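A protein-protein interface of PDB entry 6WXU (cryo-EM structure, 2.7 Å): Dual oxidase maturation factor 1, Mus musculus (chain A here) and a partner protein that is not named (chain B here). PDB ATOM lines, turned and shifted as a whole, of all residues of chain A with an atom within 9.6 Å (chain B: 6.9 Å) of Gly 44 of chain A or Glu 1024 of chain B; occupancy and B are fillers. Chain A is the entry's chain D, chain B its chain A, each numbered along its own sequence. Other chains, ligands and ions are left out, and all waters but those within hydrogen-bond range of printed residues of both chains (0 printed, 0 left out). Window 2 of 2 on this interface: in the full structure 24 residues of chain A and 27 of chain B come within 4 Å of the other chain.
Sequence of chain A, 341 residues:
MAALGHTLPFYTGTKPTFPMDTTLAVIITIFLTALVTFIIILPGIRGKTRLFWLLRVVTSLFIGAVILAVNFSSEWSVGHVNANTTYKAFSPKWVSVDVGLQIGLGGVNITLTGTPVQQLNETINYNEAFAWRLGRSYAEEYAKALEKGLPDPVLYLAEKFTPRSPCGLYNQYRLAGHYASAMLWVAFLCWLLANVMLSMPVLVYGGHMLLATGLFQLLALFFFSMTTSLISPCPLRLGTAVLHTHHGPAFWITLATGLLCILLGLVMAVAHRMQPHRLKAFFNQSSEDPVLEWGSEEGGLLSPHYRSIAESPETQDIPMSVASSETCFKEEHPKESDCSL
Thr 37 of chain A touches none of the printed residues of chain B.
Of the printed residues of chain B, Ile 41 of chain A touches Ile 1023 (3.9 Å) and Arg 1027 (3.7 Å).
Of the printed residues of chain B, Pro 43 of chain A touches Lys 1020.
Gly 44 of chain A touches just these residues of chain B: Ile 1023 (3.7 Å), Glu 1024 (3.5 Å) and Arg 1027 (3.3 Å).
Of the printed residues of chain B, Arg 50 of chain A touches Lys 1020.
Phe 1019 of chain B touches none of the printed residues of chain A.
Of the printed residues of chain A, Lys 1020 of chain B touches Pro 43 (3.4 Å) and Arg 50 (3.8 Å).
Printed residues of chain A within 4 Å of Ile 1023 of chain B: Ile 41 and Gly 44.
Of the printed residues of chain A, Glu 1024 of chain B touches Gly 44.
The nearest printed residue of chain A that does not touch Ile 1023 of chain B is Ile 40 of chain A (4.003 Å).
Of the 12 printed residues of chain B, 4 touch a printed residue of chain A.
Printed residues of chain B that touch a printed residue of chain A: Lys 1020, Ile 1023, Glu 1024 and Arg 1027.
Hydrophobic or aromatic side chains of chain B within 4 Å of the printed part of chain A: Ile 1023.
Along chain B the printed residues that touch a printed residue of chain A span positions 1020 to 1027.
Of the 14 printed residues of chain A, 4 touch a printed residue of chain B.
Hydrophobic or aromatic side chains of chain A that line the printed part of chain B: Ile 41.
NZ of Lys 1020 of chain B is in salt-bridge range of OE1 of Glu 1024 of chain B, at 3.9 Å.
Among the printed residues, merely in contact across the chains: Gly 44 of chain A with Arg 1027 of chain B, Pro 43 of chain A with Lys 1020 of chain B, Gly 44 of chain A with Glu 1024 of chain B, Gly 44 of chain A with Ile 1023 of chain B, Ile 41 of chain A with Arg 1027 of chain B, Arg 50 of chain A with Lys 1020 of chain B and Ile 41 of chain A with Ile 1023 of chain B.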
ATOM      1  N   THR A  37     -19.685  -2.609  32.666  1.00  0.00           N
ATOM      2  CA  THR A  37     -21.097  -2.875  32.931  1.00  0.00           C
ATOM      3  C   THR A  37     -21.784  -3.460  31.704  1.00  0.00           C
ATOM      4  O   THR A  37     -22.516  -4.454  31.797  1.00  0.00           O
ATOM      5  CB  THR A  37     -21.802  -1.593  33.373  1.00  0.00           C
ATOM      6  OG1 THR A  37     -21.293  -1.181  34.647  1.00  0.00           O
ATOM      7  CG2 THR A  37     -23.296  -1.821  33.481  1.00  0.00           C
ATOM      8  N   PHE A  38     -21.557  -2.856  30.537  1.00  0.00           N
ATOM      9  CA  PHE A  38     -22.212  -3.361  29.336  1.00  0.00           C
ATOM     10  C   PHE A  38     -21.656  -4.715  28.915  1.00  0.00           C
ATOM     11  O   PHE A  38     -22.392  -5.532  28.352  1.00  0.00           O
ATOM     12  CB  PHE A  38     -22.100  -2.340  28.211  1.00  0.00           C
ATOM     13  CG  PHE A  38     -22.981  -1.138  28.407  1.00  0.00           C
ATOM     14  CD1 PHE A  38     -24.254  -1.280  28.935  1.00  0.00           C
ATOM     15  CD2 PHE A  38     -22.536   0.130  28.086  1.00  0.00           C
ATOM     16  CE1 PHE A  38     -25.068  -0.181  29.127  1.00  0.00           C
ATOM     17  CE2 PHE A  38     -23.348   1.234  28.277  1.00  0.00           C
ATOM     18  CZ  PHE A  38     -24.615   1.076  28.799  1.00  0.00           C
ATOM     19  N   ILE A  39     -20.381  -4.989  29.194  1.00  0.00           N
ATOM     20  CA  ILE A  39     -19.845  -6.322  28.927  1.00  0.00           C
ATOM     21  C   ILE A  39     -20.511  -7.353  29.827  1.00  0.00           C
ATOM     22  O   ILE A  39     -20.763  -8.492  29.415  1.00  0.00           O
ATOM     23  CB  ILE A  39     -18.315  -6.330  29.091  1.00  0.00           C
ATOM     24  CG1 ILE A  39     -17.650  -5.598  27.924  1.00  0.00           C
ATOM     25  CG2 ILE A  39     -17.787  -7.750  29.191  1.00  0.00           C
ATOM     26  CD1 ILE A  39     -16.145  -5.644  27.966  1.00  0.00           C
ATOM     27  N   ILE A  40     -20.813  -6.970  31.068  1.00  0.00           N
ATOM     28  CA  ILE A  40     -21.510  -7.874  31.979  1.00  0.00           C
ATOM     29  C   ILE A  40     -22.915  -8.170  31.469  1.00  0.00           C
ATOM     30  O   ILE A  40     -23.380  -9.313  31.518  1.00  0.00           O
ATOM     31  CB  ILE A  40     -21.541  -7.282  33.400  1.00  0.00           C
ATOM     32  CG1 ILE A  40     -20.144  -7.285  34.014  1.00  0.00           C
ATOM     33  CG2 ILE A  40     -22.502  -8.052  34.280  1.00  0.00           C
ATOM     34  CD1 ILE A  40     -20.106  -6.707  35.401  1.00  0.00           C
ATOM     35  N   ILE A  41     -23.610  -7.146  30.970  1.00  0.00           N
ATOM     36  CA  ILE A  41     -24.956  -7.339  30.441  1.00  0.00           C
ATOM     37  C   ILE A  41     -24.954  -8.099  29.120  1.00  0.00           C
ATOM     38  O   ILE A  41     -25.941  -8.765  28.791  1.00  0.00           O
ATOM     39  CB  ILE A  41     -25.655  -5.975  30.281  1.00  0.00           C
ATOM     40  CG1 ILE A  41     -25.766  -5.277  31.629  1.00  0.00           C
ATOM     41  CG2 ILE A  41     -27.036  -6.123  29.676  1.00  0.00           C
ATOM     42  CD1 ILE A  41     -26.553  -4.002  31.574  1.00  0.00           C
ATOM     43  N   LEU A  42     -23.856  -8.048  28.369  1.00  0.00           N
ATOM     44  CA  LEU A  42     -23.825  -8.588  27.009  1.00  0.00           C
ATOM     45  C   LEU A  42     -24.342 -10.017  26.869  1.00  0.00           C
ATOM     46  O   LEU A  42     -25.107 -10.274  25.927  1.00  0.00           O
ATOM     47  CB  LEU A  42     -22.396  -8.479  26.462  1.00  0.00           C
ATOM     48  CG  LEU A  42     -22.253  -8.751  24.970  1.00  0.00           C
ATOM     49  CD1 LEU A  42     -22.980  -7.682  24.184  1.00  0.00           C
ATOM     50  CD2 LEU A  42     -20.791  -8.809  24.583  1.00  0.00           C
ATOM     51  N   PRO A  43     -23.976 -10.992  27.728  1.00  0.00           N
ATOM     52  CA  PRO A  43     -24.459 -12.365  27.503  1.00  0.00           C
ATOM     53  C   PRO A  43     -25.966 -12.519  27.626  1.00  0.00           C
ATOM     54  O   PRO A  43     -26.499 -13.616  27.436  1.00  0.00           O
ATOM     55  CB  PRO A  43     -23.733 -13.173  28.586  1.00  0.00           C
ATOM     56  CG  PRO A  43     -22.527 -12.384  28.890  1.00  0.00           C
ATOM     57  CD  PRO A  43     -22.969 -10.958  28.802  1.00  0.00           C
ATOM     58  N   GLY A  44     -26.667 -11.434  27.938  1.00  0.00           N
ATOM     59  CA  GLY A  44     -28.110 -11.482  28.048  1.00  0.00           C
ATOM     60  C   GLY A  44     -28.823 -10.897  26.848  1.00  0.00           C
ATOM     61  O   GLY A  44     -29.952 -10.411  26.966  1.00  0.00           O
ATOM     62  N   ILE A  45     -28.176 -10.935  25.684  1.00  0.00           N
ATOM     63  CA  ILE A  45     -28.752 -10.432  24.445  1.00  0.00           C
ATOM     64  C   ILE A  45     -28.672 -11.539  23.402  1.00  0.00           C
ATOM     65  O   ILE A  45     -27.833 -12.439  23.482  1.00  0.00           O
ATOM     66  CB  ILE A  45     -28.042  -9.152  23.948  1.00  0.00           C
ATOM     67  CG1 ILE A  45     -27.791  -8.199  25.114  1.00  0.00           C
ATOM     68  CG2 ILE A  45     -28.881  -8.437  22.910  1.00  0.00           C
ATOM     69  CD1 ILE A  45     -27.248  -6.860  24.702  1.00  0.00           C
ATOM     70  N   ARG A  46     -29.573 -11.471  22.423  1.00  0.00           N
ATOM     71  CA  ARG A  46     -29.617 -12.469  21.363  1.00  0.00           C
ATOM     72  C   ARG A  46     -28.267 -12.571  20.659  1.00  0.00           C
ATOM     73  O   ARG A  46     -27.493 -11.613  20.608  1.00  0.00           O
ATOM     74  CB  ARG A  46     -30.711 -12.120  20.352  1.00  0.00           C
ATOM     75  N   GLY A  47     -27.991 -13.756  20.110  1.00  0.00           N
ATOM     76  CA  GLY A  47     -26.680 -14.008  19.537  1.00  0.00           C
ATOM     77  C   GLY A  47     -26.391 -13.208  18.284  1.00  0.00           C
ATOM     78  O   GLY A  47     -25.231 -12.886  18.005  1.00  0.00           O
ATOM     79  N   THR A  49     -27.579  -9.997  17.269  1.00  0.00           N
ATOM     80  CA  THR A  49     -27.355  -8.573  17.476  1.00  0.00           C
ATOM     81  C   THR A  49     -26.254  -8.275  18.486  1.00  0.00           C
ATOM     82  O   THR A  49     -26.128  -7.121  18.910  1.00  0.00           O
ATOM     83  CB  THR A  49     -28.651  -7.894  17.923  1.00  0.00           C
ATOM     84  OG1 THR A  49     -29.023  -8.378  19.219  1.00  0.00           O
ATOM     85  CG2 THR A  49     -29.770  -8.186  16.938  1.00  0.00           C
ATOM     86  N   ARG A  50     -25.453  -9.270  18.874  1.00  0.00           N
ATOM     87  CA  ARG A  50     -24.376  -9.014  19.824  1.00  0.00           C
ATOM     88  C   ARG A  50     -23.351  -8.045  19.248  1.00  0.00           C
ATOM     89  O   ARG A  50     -22.970  -7.069  19.903  1.00  0.00           O
ATOM     90  CB  ARG A  50     -23.707 -10.324  20.234  1.00  0.00           C
ATOM     91  CG  ARG A  50     -24.454 -11.077  21.314  1.00  0.00           C
ATOM     92  CD  ARG A  50     -23.718 -12.334  21.723  1.00  0.00           C
ATOM     93  NE  ARG A  50     -24.459 -13.086  22.728  1.00  0.00           N
ATOM     94  CZ  ARG A  50     -24.071 -14.255  23.222  1.00  0.00           C
ATOM     95  NH1 ARG A  50     -22.942 -14.812  22.807  1.00  0.00           N
ATOM     96  NH2 ARG A  50     -24.811 -14.868  24.135  1.00  0.00           N
ATOM     97  N   TRP A  53     -24.791  -4.538  18.793  1.00  0.00           N
ATOM     98  CA  TRP A  53     -24.857  -3.751  20.017  1.00  0.00           C
ATOM     99  C   TRP A  53     -23.470  -3.363  20.499  1.00  0.00           C
ATOM    100  O   TRP A  53     -23.271  -2.242  20.981  1.00  0.00           O
ATOM    101  CB  TRP A  53     -25.596  -4.520  21.106  1.00  0.00           C
ATOM    102  CG  TRP A  53     -27.037  -4.172  21.186  1.00  0.00           C
ATOM    103  CD1 TRP A  53     -28.085  -4.910  20.733  1.00  0.00           C
ATOM    104  CD2 TRP A  53     -27.596  -2.982  21.748  1.00  0.00           C
ATOM    105  NE1 TRP A  53     -29.267  -4.259  20.983  1.00  0.00           N
ATOM    106  CE2 TRP A  53     -28.993  -3.070  21.606  1.00  0.00           C
ATOM    107  CE3 TRP A  53     -27.052  -1.851  22.361  1.00  0.00           C
ATOM    108  CZ2 TRP A  53     -29.851  -2.072  22.054  1.00  0.00           C
ATOM    109  CZ3 TRP A  53     -27.904  -0.862  22.806  1.00  0.00           C
ATOM    110  CH2 TRP A  53     -29.288  -0.979  22.651  1.00  0.00           C
ATOM    111  N   GLN B1017     -26.206 -22.125  29.619  1.00  0.00           N
ATOM    112  CA  GLN B1017     -27.485 -21.650  29.102  1.00  0.00           C
ATOM    113  C   GLN B1017     -28.346 -21.093  30.225  1.00  0.00           C
ATOM    114  O   GLN B1017     -28.989 -20.048  30.067  1.00  0.00           O
ATOM    115  CB  GLN B1017     -28.211 -22.782  28.376  1.00  0.00           C
ATOM    116  CG  GLN B1017     -27.364 -23.522  27.349  1.00  0.00           C
ATOM    117  CD  GLN B1017     -26.472 -24.580  27.975  1.00  0.00           C
ATOM    118  OE1 GLN B1017     -26.484 -24.782  29.189  1.00  0.00           O
ATOM    119  NE2 GLN B1017     -25.687 -25.258  27.145  1.00  0.00           N
ATOM    120  N   PHE B1019     -27.114 -19.782  32.857  1.00  0.00           N
ATOM    121  CA  PHE B1019     -26.454 -18.536  33.232  1.00  0.00           C
ATOM    122  C   PHE B1019     -26.934 -17.377  32.370  1.00  0.00           C
ATOM    123  O   PHE B1019     -27.343 -16.331  32.888  1.00  0.00           O
ATOM    124  CB  PHE B1019     -24.940 -18.697  33.126  1.00  0.00           C
ATOM    125  CG  PHE B1019     -24.187 -17.402  33.171  1.00  0.00           C
ATOM    126  CD1 PHE B1019     -23.976 -16.753  34.372  1.00  0.00           C
ATOM    127  CD2 PHE B1019     -23.683 -16.837  32.012  1.00  0.00           C
ATOM    128  CE1 PHE B1019     -23.280 -15.563  34.418  1.00  0.00           C
ATOM    129  CE2 PHE B1019     -22.987 -15.647  32.052  1.00  0.00           C
ATOM    130  CZ  PHE B1019     -22.785 -15.010  33.256  1.00  0.00           C
ATOM    131  N   LYS B1020     -26.888 -17.540  31.048  1.00  0.00           N
ATOM    132  CA  LYS B1020     -27.331 -16.456  30.180  1.00  0.00           C
ATOM    133  C   LYS B1020     -28.830 -16.215  30.305  1.00  0.00           C
ATOM    134  O   LYS B1020     -29.290 -15.084  30.113  1.00  0.00           O
ATOM    135  CB  LYS B1020     -26.939 -16.739  28.730  1.00  0.00           C
ATOM    136  CG  LYS B1020     -27.315 -18.112  28.228  1.00  0.00           C
ATOM    137  CD  LYS B1020     -26.680 -18.383  26.875  1.00  0.00           C
ATOM    138  CE  LYS B1020     -27.115 -17.356  25.843  1.00  0.00           C
ATOM    139  NZ  LYS B1020     -28.591 -17.350  25.652  1.00  0.00           N
ATOM    140  N   ARG B1021     -29.602 -17.250  30.647  1.00  0.00           N
ATOM    141  CA  ARG B1021     -31.016 -17.041  30.938  1.00  0.00           C
ATOM    142  C   ARG B1021     -31.192 -16.153  32.163  1.00  0.00           C
ATOM    143  O   ARG B1021     -32.022 -15.236  32.163  1.00  0.00           O
ATOM    144  CB  ARG B1021     -31.714 -18.384  31.141  1.00  0.00           C
ATOM    145  N   PHE B1022     -30.417 -16.411  33.217  1.00  0.00           N
ATOM    146  CA  PHE B1022     -30.456 -15.553  34.396  1.00  0.00           C
ATOM    147  C   PHE B1022     -30.077 -14.120  34.046  1.00  0.00           C
ATOM    148  O   PHE B1022     -30.712 -13.167  34.516  1.00  0.00           O
ATOM    149  CB  PHE B1022     -29.523 -16.115  35.468  1.00  0.00           C
ATOM    150  CG  PHE B1022     -29.278 -15.180  36.615  1.00  0.00           C
ATOM    151  CD1 PHE B1022     -30.181 -15.089  37.656  1.00  0.00           C
ATOM    152  CD2 PHE B1022     -28.134 -14.405  36.660  1.00  0.00           C
ATOM    153  CE1 PHE B1022     -29.953 -14.236  38.712  1.00  0.00           C
ATOM    154  CE2 PHE B1022     -27.902 -13.550  37.713  1.00  0.00           C
ATOM    155  CZ  PHE B1022     -28.811 -13.466  38.740  1.00  0.00           C
ATOM    156  N   ILE B1023     -29.044 -13.949  33.220  1.00  0.00           N
ATOM    157  CA  ILE B1023     -28.593 -12.607  32.864  1.00  0.00           C
ATOM    158  C   ILE B1023     -29.683 -11.861  32.106  1.00  0.00           C
ATOM    159  O   ILE B1023     -29.989 -10.699  32.399  1.00  0.00           O
ATOM    160  CB  ILE B1023     -27.292 -12.671  32.047  1.00  0.00           C
ATOM    161  CG1 ILE B1023     -26.183 -13.346  32.850  1.00  0.00           C
ATOM    162  CG2 ILE B1023     -26.865 -11.278  31.645  1.00  0.00           C
ATOM    163  CD1 ILE B1023     -25.781 -12.585  34.085  1.00  0.00           C
ATOM    164  N   GLU B1024     -30.282 -12.516  31.108  1.00  0.00           N
ATOM    165  CA  GLU B1024     -31.315 -11.855  30.322  1.00  0.00           C
ATOM    166  C   GLU B1024     -32.600 -11.660  31.113  1.00  0.00           C
ATOM    167  O   GLU B1024     -33.416 -10.811  30.743  1.00  0.00           O
ATOM    168  CB  GLU B1024     -31.595 -12.643  29.046  1.00  0.00           C
ATOM    169  CG  GLU B1024     -32.278 -13.972  29.273  1.00  0.00           C
ATOM    170  CD  GLU B1024     -32.158 -14.887  28.077  1.00  0.00           C
ATOM    171  OE1 GLU B1024     -31.059 -14.952  27.488  1.00  0.00           O
ATOM    172  OE2 GLU B1024     -33.163 -15.537  27.720  1.00  0.00           O
ATOM    173  N   ASN B1025     -32.798 -12.423  32.188  1.00  0.00           N
ATOM    174  CA  ASN B1025     -33.935 -12.174  33.066  1.00  0.00           C
ATOM    175  C   ASN B1025     -33.716 -10.925  33.909  1.00  0.00           C
ATOM    176  O   ASN B1025     -34.604 -10.073  34.018  1.00  0.00           O
ATOM    177  CB  ASN B1025     -34.183 -13.382  33.966  1.00  0.00           C
ATOM    178  CG  ASN B1025     -34.817 -14.533  33.227  1.00  0.00           C
ATOM    179  OD1 ASN B1025     -35.560 -14.332  32.269  1.00  0.00           O
ATOM    180  ND2 ASN B1025     -34.531 -15.751  33.669  1.00  0.00           N
ATOM    181  N   TYR B1026     -32.537 -10.798  34.517  1.00  0.00           N
ATOM    182  CA  TYR B1026     -32.277  -9.737  35.480  1.00  0.00           C
ATOM    183  C   TYR B1026     -31.353  -8.655  34.929  1.00  0.00           C
ATOM    184  O   TYR B1026     -30.574  -8.064  35.680  1.00  0.00           O
ATOM    185  CB  TYR B1026     -31.701 -10.321  36.765  1.00  0.00           C
ATOM    186  CG  TYR B1026     -32.640 -11.264  37.473  1.00  0.00           C
ATOM    187  CD1 TYR B1026     -33.557 -10.794  38.398  1.00  0.00           C
ATOM    188  CD2 TYR B1026     -32.614 -12.625  37.212  1.00  0.00           C
ATOM    189  CE1 TYR B1026     -34.418 -11.649  39.045  1.00  0.00           C
ATOM    190  CE2 TYR B1026     -33.472 -13.490  37.856  1.00  0.00           C
ATOM    191  CZ  TYR B1026     -34.371 -12.997  38.772  1.00  0.00           C
ATOM    192  OH  TYR B1026     -35.230 -13.853  39.419  1.00  0.00           O
ATOM    193  N   ARG B1027     -31.409  -8.408  33.620  1.00  0.00           N
ATOM    194  CA  ARG B1027     -30.659  -7.299  33.032  1.00  0.00           C
ATOM    195  C   ARG B1027     -30.929  -5.982  33.751  1.00  0.00           C
ATOM    196  O   ARG B1027     -30.000  -5.226  34.056  1.00  0.00           O
ATOM    197  CB  ARG B1027     -30.995  -7.175  31.547  1.00  0.00           C
ATOM    198  CG  ARG B1027     -30.110  -8.026  30.662  1.00  0.00           C
ATOM    199  CD  ARG B1027     -30.673  -8.210  29.266  1.00  0.00           C
ATOM    200  NE  ARG B1027     -30.914  -6.944  28.585  1.00  0.00           N
ATOM    201  CZ  ARG B1027     -32.120  -6.481  28.286  1.00  0.00           C
ATOM    202  NH1 ARG B1027     -32.253  -5.318  27.664  1.00  0.00           N
ATOM    203  NH2 ARG B1027     -33.196  -7.185  28.604  1.00  0.00           N
ATOM    204  N   ARG B1028     -32.199  -5.691  34.034  1.00  0.00           N
ATOM    205  CA  ARG B1028     -32.537  -4.418  34.664  1.00  0.00           C
ATOM    206  C   ARG B1028     -32.029  -4.352  36.099  1.00  0.00           C
ATOM    207  O   ARG B1028     -31.510  -3.315  36.536  1.00  0.00           O
ATOM    208  CB  ARG B1028     -34.046  -4.203  34.620  1.00  0.00           C
ATOM    209  CG  ARG B1028     -34.630  -4.168  33.225  1.00  0.00           C
ATOM    210  CD  ARG B1028     -36.124  -3.944  33.274  1.00  0.00           C
ATOM    211  NE  ARG B1028     -36.814  -5.040  33.943  1.00  0.00           N
ATOM    212  CZ  ARG B1028     -38.115  -5.051  34.213  1.00  0.00           C
ATOM    213  NH1 ARG B1028     -38.659  -6.092  34.823  1.00  0.00           N
ATOM    214  NH2 ARG B1028     -38.871  -4.018  33.871  1.00  0.00           N
ATOM    215  N   ILE B1030     -29.446  -5.942  37.332  1.00  0.00           N
ATOM    216  CA  ILE B1030     -27.997  -5.797  37.263  1.00  0.00           C
ATOM    217  C   ILE B1030     -27.619  -4.360  36.947  1.00  0.00           C
ATOM    218  O   ILE B1030     -26.702  -3.799  37.555  1.00  0.00           O
ATOM    219  CB  ILE B1030     -27.417  -6.775  36.228  1.00  0.00           C
ATOM    220  CG1 ILE B1030     -27.558  -8.210  36.727  1.00  0.00           C
ATOM    221  CG2 ILE B1030     -25.975  -6.433  35.921  1.00  0.00           C
ATOM    222  CD1 ILE B1030     -27.062  -9.237  35.753  1.00  0.00           C
